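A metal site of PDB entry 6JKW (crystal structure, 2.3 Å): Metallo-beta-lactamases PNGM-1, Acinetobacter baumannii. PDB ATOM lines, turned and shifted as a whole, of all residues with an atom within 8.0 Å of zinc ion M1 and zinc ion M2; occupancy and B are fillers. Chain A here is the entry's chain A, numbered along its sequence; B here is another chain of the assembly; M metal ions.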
ATOM      1  N   GLY A  38      -3.246   7.472   8.036  1.00  0.00           N
ATOM      2  CA  GLY A  38      -3.108   8.022   9.375  1.00  0.00           C
ATOM      3  C   GLY A  38      -4.331   8.751   9.874  1.00  0.00           C
ATOM      4  O   GLY A  38      -5.420   8.287   9.673  1.00  0.00           O
ATOM      5  N   MET A  39      -4.102   9.894  10.504  1.00  0.00           N
ATOM      6  CA  MET A  39      -5.014  10.538  11.473  1.00  0.00           C
ATOM      7  C   MET A  39      -4.968  11.998  11.152  1.00  0.00           C
ATOM      8  O   MET A  39      -4.176  12.407  10.285  1.00  0.00           O
ATOM      9  CB  MET A  39      -4.376  10.447  12.848  1.00  0.00           C
ATOM     10  CG  MET A  39      -4.236   9.045  13.425  1.00  0.00           C
ATOM     11  SD  MET A  39      -5.970   8.414  14.124  1.00  0.00           S
ATOM     12  CE  MET A  39      -6.512   9.854  15.369  1.00  0.00           C
ATOM     13  N   PRO A  40      -5.758  12.832  11.866  1.00  0.00           N
ATOM     14  CA  PRO A  40      -5.606  14.284  11.603  1.00  0.00           C
ATOM     15  C   PRO A  40      -4.370  14.923  12.255  1.00  0.00           C
ATOM     16  O   PRO A  40      -4.157  16.126  12.127  1.00  0.00           O
ATOM     17  CB  PRO A  40      -6.906  14.865  12.179  1.00  0.00           C
ATOM     18  CG  PRO A  40      -7.344  13.870  13.193  1.00  0.00           C
ATOM     19  CD  PRO A  40      -6.966  12.537  12.629  1.00  0.00           C
ATOM     20  N   ALA A  48      -2.042  11.471   5.899  1.00  0.00           N
ATOM     21  CA  ALA A  48      -3.478  11.301   6.160  1.00  0.00           C
ATOM     22  C   ALA A  48      -4.122  10.581   4.973  1.00  0.00           C
ATOM     23  O   ALA A  48      -3.562  10.593   3.859  1.00  0.00           O
ATOM     24  CB  ALA A  48      -4.146  12.638   6.364  1.00  0.00           C
ATOM     25  N   ALA A  49      -5.309  10.053   5.174  1.00  0.00           N
ATOM     26  CA  ALA A  49      -5.944   9.162   4.212  1.00  0.00           C
ATOM     27  C   ALA A  49      -5.854   9.571   2.733  1.00  0.00           C
ATOM     28  O   ALA A  49      -6.178  10.715   2.379  1.00  0.00           O
ATOM     29  CB  ALA A  49      -7.401   9.024   4.570  1.00  0.00           C
ATOM     30  N   ASP A  64      -9.901  10.152  -1.573  1.00  0.00           N
ATOM     31  CA  ASP A  64      -9.352  10.966  -0.473  1.00  0.00           C
ATOM     32  C   ASP A  64      -7.957  11.425  -0.774  1.00  0.00           C
ATOM     33  O   ASP A  64      -7.217  10.742  -1.396  1.00  0.00           O
ATOM     34  CB  ASP A  64      -9.492  10.248   0.914  1.00  0.00           C
ATOM     35  CG  ASP A  64     -10.928  10.199   1.405  1.00  0.00           C
ATOM     36  OD1 ASP A  64     -11.767  10.960   0.805  1.00  0.00           O
ATOM     37  OD2 ASP A  64     -11.240   9.384   2.325  1.00  0.00           O
ATOM     38  N   THR A  89     -14.507  11.078   0.419  1.00  0.00           N
ATOM     39  CA  THR A  89     -15.465  10.495   1.339  1.00  0.00           C
ATOM     40  C   THR A  89     -16.126  11.528   2.254  1.00  0.00           C
ATOM     41  O   THR A  89     -17.286  11.408   2.591  1.00  0.00           O
ATOM     42  CB  THR A  89     -14.825   9.479   2.266  1.00  0.00           C
ATOM     43  OG1 THR A  89     -13.808  10.107   3.057  1.00  0.00           O
ATOM     44  CG2 THR A  89     -14.362   8.244   1.503  1.00  0.00           C
ATOM     45  N   HIS A  90     -15.360  12.507   2.706  1.00  0.00           N
ATOM     46  CA  HIS A  90     -15.902  13.596   3.521  1.00  0.00           C
ATOM     47  C   HIS A  90     -14.944  14.710   3.651  1.00  0.00           C
ATOM     48  O   HIS A  90     -13.840  14.611   3.177  1.00  0.00           O
ATOM     49  CB  HIS A  90     -16.317  13.123   4.906  1.00  0.00           C
ATOM     50  CG  HIS A  90     -15.204  12.556   5.730  1.00  0.00           C
ATOM     51  ND1 HIS A  90     -14.463  11.466   5.326  1.00  0.00           N
ATOM     52  CD2 HIS A  90     -14.753  12.887   6.950  1.00  0.00           C
ATOM     53  CE1 HIS A  90     -13.591  11.160   6.269  1.00  0.00           C
ATOM     54  NE2 HIS A  90     -13.765  11.998   7.271  1.00  0.00           N
ATOM     55  N   LEU A  91     -15.333  15.756   4.358  1.00  0.00           N
ATOM     56  CA  LEU A  91     -14.688  17.046   4.244  1.00  0.00           C
ATOM     57  C   LEU A  91     -13.818  17.431   5.428  1.00  0.00           C
ATOM     58  O   LEU A  91     -13.469  18.596   5.636  1.00  0.00           O
ATOM     59  CB  LEU A  91     -15.796  18.078   3.933  1.00  0.00           C
ATOM     60  CG  LEU A  91     -16.549  17.905   2.599  1.00  0.00           C
ATOM     61  CD1 LEU A  91     -17.602  18.993   2.505  1.00  0.00           C
ATOM     62  CD2 LEU A  91     -15.613  18.078   1.404  1.00  0.00           C
ATOM     63  N   HIS A  92     -13.385  16.423   6.186  1.00  0.00           N
ATOM     64  CA  HIS A  92     -12.326  16.653   7.168  1.00  0.00           C
ATOM     65  C   HIS A  92     -11.025  16.891   6.458  1.00  0.00           C
ATOM     66  O   HIS A  92     -10.746  16.265   5.458  1.00  0.00           O
ATOM     67  CB  HIS A  92     -12.086  15.455   8.083  1.00  0.00           C
ATOM     68  CG  HIS A  92     -12.949  15.401   9.291  1.00  0.00           C
ATOM     69  ND1 HIS A  92     -13.533  14.244   9.714  1.00  0.00           N
ATOM     70  CD2 HIS A  92     -13.271  16.342  10.197  1.00  0.00           C
ATOM     71  CE1 HIS A  92     -14.232  14.478  10.820  1.00  0.00           C
ATOM     72  NE2 HIS A  92     -14.098  15.753  11.115  1.00  0.00           N
ATOM     73  N   THR A  93     -10.214  17.746   7.049  1.00  0.00           N
ATOM     74  CA  THR A  93      -8.879  18.082   6.574  1.00  0.00           C
ATOM     75  C   THR A  93      -8.010  16.848   6.315  1.00  0.00           C
ATOM     76  O   THR A  93      -7.260  16.816   5.333  1.00  0.00           O
ATOM     77  CB  THR A  93      -8.172  19.059   7.567  1.00  0.00           C
ATOM     78  OG1 THR A  93      -7.725  18.349   8.707  1.00  0.00           O
ATOM     79  CG2 THR A  93      -9.160  20.148   8.042  1.00  0.00           C
ATOM     80  N   ASP A  94      -8.095  15.821   7.130  1.00  0.00           N
ATOM     81  CA  ASP A  94      -7.231  14.672   6.912  1.00  0.00           C
ATOM     82  C   ASP A  94      -7.741  13.785   5.765  1.00  0.00           C
ATOM     83  O   ASP A  94      -7.204  12.674   5.506  1.00  0.00           O
ATOM     84  CB  ASP A  94      -7.048  13.887   8.214  1.00  0.00           C
ATOM     85  CG  ASP A  94      -8.335  13.402   8.785  1.00  0.00           C
ATOM     86  OD1 ASP A  94      -8.549  12.143   8.960  1.00  0.00           O
ATOM     87  OD2 ASP A  94      -9.151  14.304   9.054  1.00  0.00           O
ATOM     88  N   HIS A  95      -8.784  14.241   5.062  1.00  0.00           N
ATOM     89  CA  HIS A  95      -9.256  13.564   3.869  1.00  0.00           C
ATOM     90  C   HIS A  95      -9.227  14.389   2.610  1.00  0.00           C
ATOM     91  O   HIS A  95      -9.292  13.807   1.531  1.00  0.00           O
ATOM     92  CB  HIS A  95     -10.646  13.055   4.118  1.00  0.00           C
ATOM     93  CG  HIS A  95     -10.628  11.899   5.043  1.00  0.00           C
ATOM     94  ND1 HIS A  95     -10.730  10.598   4.601  1.00  0.00           N
ATOM     95  CD2 HIS A  95     -10.366  11.833   6.361  1.00  0.00           C
ATOM     96  CE1 HIS A  95     -10.602   9.784   5.636  1.00  0.00           C
ATOM     97  NE2 HIS A  95     -10.350  10.512   6.692  1.00  0.00           N
ATOM     98  N   HIS A 187     -20.603   9.922  11.208  1.00  0.00           N
ATOM     99  CA  HIS A 187     -19.320  10.486  11.580  1.00  0.00           C
ATOM    100  C   HIS A 187     -19.375  12.011  11.662  1.00  0.00           C
ATOM    101  O   HIS A 187     -19.427  12.685  10.636  1.00  0.00           O
ATOM    102  CB  HIS A 187     -18.368  10.055  10.503  1.00  0.00           C
ATOM    103  CG  HIS A 187     -17.007  10.644  10.591  1.00  0.00           C
ATOM    104  ND1 HIS A 187     -16.056  10.203  11.481  1.00  0.00           N
ATOM    105  CD2 HIS A 187     -16.412  11.582   9.833  1.00  0.00           C
ATOM    106  CE1 HIS A 187     -14.956  10.902  11.310  1.00  0.00           C
ATOM    107  NE2 HIS A 187     -15.134  11.718  10.283  1.00  0.00           N
ATOM    108  N   ALA A 188     -19.414  12.542  12.898  1.00  0.00           N
ATOM    109  CA  ALA A 188     -19.323  13.983  13.228  1.00  0.00           C
ATOM    110  C   ALA A 188     -20.588  14.806  12.899  1.00  0.00           C
ATOM    111  O   ALA A 188     -20.919  15.738  13.634  1.00  0.00           O
ATOM    112  CB  ALA A 188     -18.112  14.614  12.563  1.00  0.00           C
ATOM    113  N   PRO A 192     -20.642  12.638   5.374  1.00  0.00           N
ATOM    114  CA  PRO A 192     -19.679  11.552   5.086  1.00  0.00           C
ATOM    115  C   PRO A 192     -20.338  10.361   4.465  1.00  0.00           C
ATOM    116  O   PRO A 192     -21.487  10.072   4.813  1.00  0.00           O
ATOM    117  CB  PRO A 192     -19.114  11.230   6.473  1.00  0.00           C
ATOM    118  CG  PRO A 192     -19.221  12.518   7.208  1.00  0.00           C
ATOM    119  CD  PRO A 192     -20.539  13.080   6.768  1.00  0.00           C
ATOM    120  N   GLY A 208     -14.054   5.146   4.153  1.00  0.00           N
ATOM    121  CA  GLY A 208     -14.091   6.478   4.770  1.00  0.00           C
ATOM    122  C   GLY A 208     -14.051   6.406   6.305  1.00  0.00           C
ATOM    123  O   GLY A 208     -13.398   5.549   6.873  1.00  0.00           O
ATOM    124  N   ASP A 209     -14.737   7.331   6.979  1.00  0.00           N
ATOM    125  CA  ASP A 209     -14.752   7.336   8.451  1.00  0.00           C
ATOM    126  C   ASP A 209     -16.184   7.117   8.848  1.00  0.00           C
ATOM    127  O   ASP A 209     -17.093   7.758   8.284  1.00  0.00           O
ATOM    128  CB  ASP A 209     -14.396   8.680   9.045  1.00  0.00           C
ATOM    129  CG  ASP A 209     -12.931   9.054   8.906  1.00  0.00           C
ATOM    130  OD1 ASP A 209     -12.108   8.241   8.440  1.00  0.00           O
ATOM    131  OD2 ASP A 209     -12.611  10.235   9.269  1.00  0.00           O
ATOM    132  N   THR A 210     -16.368   6.261   9.847  1.00  0.00           N
ATOM    133  CA  THR A 210     -17.702   5.982  10.369  1.00  0.00           C
ATOM    134  C   THR A 210     -17.649   5.162  11.676  1.00  0.00           C
ATOM    135  O   THR A 210     -16.723   4.334  11.873  1.00  0.00           O
ATOM    136  CB  THR A 210     -18.531   5.216   9.308  1.00  0.00           C
ATOM    137  OG1 THR A 210     -19.921   5.157   9.702  1.00  0.00           O
ATOM    138  CG2 THR A 210     -17.921   3.819   9.044  1.00  0.00           C
ATOM    139  N   GLU A 229     -12.499   1.954   8.589  1.00  0.00           N
ATOM    140  CA  GLU A 229     -11.909   2.499   9.788  1.00  0.00           C
ATOM    141  C   GLU A 229     -11.862   1.449  10.908  1.00  0.00           C
ATOM    142  O   GLU A 229     -12.797   0.677  11.108  1.00  0.00           O
ATOM    143  CB  GLU A 229     -12.701   3.756  10.190  1.00  0.00           C
ATOM    144  CG  GLU A 229     -13.269   3.777  11.613  1.00  0.00           C
ATOM    145  CD  GLU A 229     -13.591   5.181  12.136  1.00  0.00           C
ATOM    146  OE1 GLU A 229     -14.094   6.058  11.373  1.00  0.00           O
ATOM    147  OE2 GLU A 229     -13.345   5.396  13.312  1.00  0.00           O
ATOM    148  N   TRP A 231     -10.343   1.748  14.880  1.00  0.00           N
ATOM    149  CA  TRP A 231      -9.723   2.764  15.751  1.00  0.00           C
ATOM    150  C   TRP A 231      -8.781   2.184  16.774  1.00  0.00           C
ATOM    151  O   TRP A 231      -8.809   1.000  17.041  1.00  0.00           O
ATOM    152  CB  TRP A 231     -10.772   3.630  16.432  1.00  0.00           C
ATOM    153  CG  TRP A 231     -10.323   4.995  16.852  1.00  0.00           C
ATOM    154  CD1 TRP A 231     -10.042   5.400  18.112  1.00  0.00           C
ATOM    155  CD2 TRP A 231     -10.184   6.161  16.035  1.00  0.00           C
ATOM    156  NE1 TRP A 231      -9.698   6.728  18.136  1.00  0.00           N
ATOM    157  CE2 TRP A 231      -9.804   7.219  16.868  1.00  0.00           C
ATOM    158  CE3 TRP A 231     -10.343   6.395  14.664  1.00  0.00           C
ATOM    159  CZ2 TRP A 231      -9.561   8.524  16.382  1.00  0.00           C
ATOM    160  CZ3 TRP A 231     -10.094   7.703  14.166  1.00  0.00           C
ATOM    161  CH2 TRP A 231      -9.716   8.741  15.034  1.00  0.00           C
ATOM    162  N   HIS A 256     -16.321   5.867  16.967  1.00  0.00           N
ATOM    163  CA  HIS A 256     -15.472   5.119  16.072  1.00  0.00           C
ATOM    164  C   HIS A 256     -15.800   3.659  16.037  1.00  0.00           C
ATOM    165  O   HIS A 256     -16.574   3.164  16.828  1.00  0.00           O
ATOM    166  CB  HIS A 256     -13.996   5.325  16.429  1.00  0.00           C
ATOM    167  CG  HIS A 256     -13.573   6.764  16.317  1.00  0.00           C
ATOM    168  ND1 HIS A 256     -13.291   7.361  15.107  1.00  0.00           N
ATOM    169  CD2 HIS A 256     -13.480   7.735  17.261  1.00  0.00           C
ATOM    170  CE1 HIS A 256     -13.021   8.642  15.311  1.00  0.00           C
ATOM    171  NE2 HIS A 256     -13.120   8.889  16.604  1.00  0.00           N
ATOM    172  N   TYR A 277      -7.595   0.467   8.533  1.00  0.00           N
ATOM    173  CA  TYR A 277      -6.718   1.643   8.466  1.00  0.00           C
ATOM    174  C   TYR A 277      -7.196   2.676   9.437  1.00  0.00           C
ATOM    175  O   TYR A 277      -8.206   2.481  10.088  1.00  0.00           O
ATOM    176  CB  TYR A 277      -6.698   2.239   6.996  1.00  0.00           C
ATOM    177  CG  TYR A 277      -7.783   3.268   6.688  1.00  0.00           C
ATOM    178  CD1 TYR A 277      -9.125   2.930   6.692  1.00  0.00           C
ATOM    179  CD2 TYR A 277      -7.456   4.577   6.393  1.00  0.00           C
ATOM    180  CE1 TYR A 277     -10.108   3.887   6.422  1.00  0.00           C
ATOM    181  CE2 TYR A 277      -8.434   5.552   6.136  1.00  0.00           C
ATOM    182  CZ  TYR A 277      -9.759   5.188   6.121  1.00  0.00           C
ATOM    183  OH  TYR A 277     -10.738   6.154   5.823  1.00  0.00           O
ATOM    184  N   HIS A 278      -6.496   3.811   9.422  1.00  0.00           N
ATOM    185  CA  HIS A 278      -6.844   5.044  10.168  1.00  0.00           C
ATOM    186  C   HIS A 278      -6.499   4.967  11.627  1.00  0.00           C
ATOM    187  O   HIS A 278      -7.120   5.593  12.480  1.00  0.00           O
ATOM    188  CB  HIS A 278      -8.308   5.378   9.958  1.00  0.00           C
ATOM    189  CG  HIS A 278      -8.604   6.847   9.957  1.00  0.00           C
ATOM    190  ND1 HIS A 278      -8.496   7.640  11.072  1.00  0.00           N
ATOM    191  CD2 HIS A 278      -9.106   7.643   8.986  1.00  0.00           C
ATOM    192  CE1 HIS A 278      -8.907   8.858  10.797  1.00  0.00           C
ATOM    193  NE2 HIS A 278      -9.283   8.890   9.531  1.00  0.00           N
ATOM    194  N   TRP B 142     -17.478  22.608   7.014  1.00  0.00           N
ATOM    195  CA  TRP B 142     -18.100  21.369   7.510  1.00  0.00           C
ATOM    196  C   TRP B 142     -17.353  20.814   8.721  1.00  0.00           C
ATOM    197  O   TRP B 142     -17.950  20.358   9.673  1.00  0.00           O
ATOM    198  CB  TRP B 142     -18.142  20.299   6.419  1.00  0.00           C
ATOM    199  CG  TRP B 142     -18.808  19.050   6.860  1.00  0.00           C
ATOM    200  CD1 TRP B 142     -20.152  18.779   6.810  1.00  0.00           C
ATOM    201  CD2 TRP B 142     -18.189  17.914   7.460  1.00  0.00           C
ATOM    202  NE1 TRP B 142     -20.390  17.547   7.357  1.00  0.00           N
ATOM    203  CE2 TRP B 142     -19.212  16.987   7.753  1.00  0.00           C
ATOM    204  CE3 TRP B 142     -16.864  17.596   7.795  1.00  0.00           C
ATOM    205  CZ2 TRP B 142     -18.979  15.800   8.366  1.00  0.00           C
ATOM    206  CZ3 TRP B 142     -16.633  16.374   8.394  1.00  0.00           C
ATOM    207  CH2 TRP B 142     -17.699  15.476   8.656  1.00  0.00           C
ATOM    208  N   ASP B 143     -16.037  20.790   8.612  1.00  0.00           N
ATOM    209  CA  ASP B 143     -15.108  20.313   9.629  1.00  0.00           C
ATOM    210  C   ASP B 143     -15.242  21.240  10.837  1.00  0.00           C
ATOM    211  O   ASP B 143     -15.352  20.778  11.959  1.00  0.00           O
ATOM    212  CB  ASP B 143     -13.669  20.336   9.001  1.00  0.00           C
ATOM    213  CG  ASP B 143     -12.559  19.744   9.921  1.00  0.00           C
ATOM    214  OD1 ASP B 143     -12.489  20.174  11.108  1.00  0.00           O
ATOM    215  OD2 ASP B 143     -11.714  18.915   9.408  1.00  0.00           O
HETATM  216 ZN    ZN M   1     -10.533  10.702   9.091  1.00  0.00          ZN
HETATM  217 ZN    ZN M   2     -13.145  12.193   9.517  1.00  0.00          ZN
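ND1 of His 278 lies within hydrogen-bond range of O of Gly 38. OG1 of Thr 89 lies within hydrogen-bond range of ND1 of His 90 (2.7 Å). The side-chain hydroxyl (OG1) of Thr 89 sits at hydrogen-bond distance from a ring nitrogen (ND1) of His 95 (3.5 Å). A ring nitrogen (ND1) of His 95 lies within hydrogen-bond range of the side-chain carboxylate of Asp 64. The backbone carbonyl oxygen (O) of Asp 94 lies within hydrogen-bond range of the backbone NH (N) of Ala 49, 3.3 Å away.
Within 4 Å of zinc ion M1: His 90, Asp 94, His 95, Asp 209 and His 278.
Of the 26 residues printed, 4 come within 4 Å of zinc ion M2. The nearest printed residue that does not touch zinc ion M2 is His 95 (4.2 Å).
Zinc ion M1 is bound by OD2 of Asp 209, NE2 of His 278, NE2 of His 95 and OD1 of Asp 94.
OD2 of Asp 209 is bound to zinc ion M2, 2.0 Å away. ND1 of His 92 binds zinc ion M2, 2.1 Å away. A ring nitrogen (NE2) of His 187 is bound to zinc ion M2. NE2 of His 90 binds zinc ion M2, at 2.3 Å.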
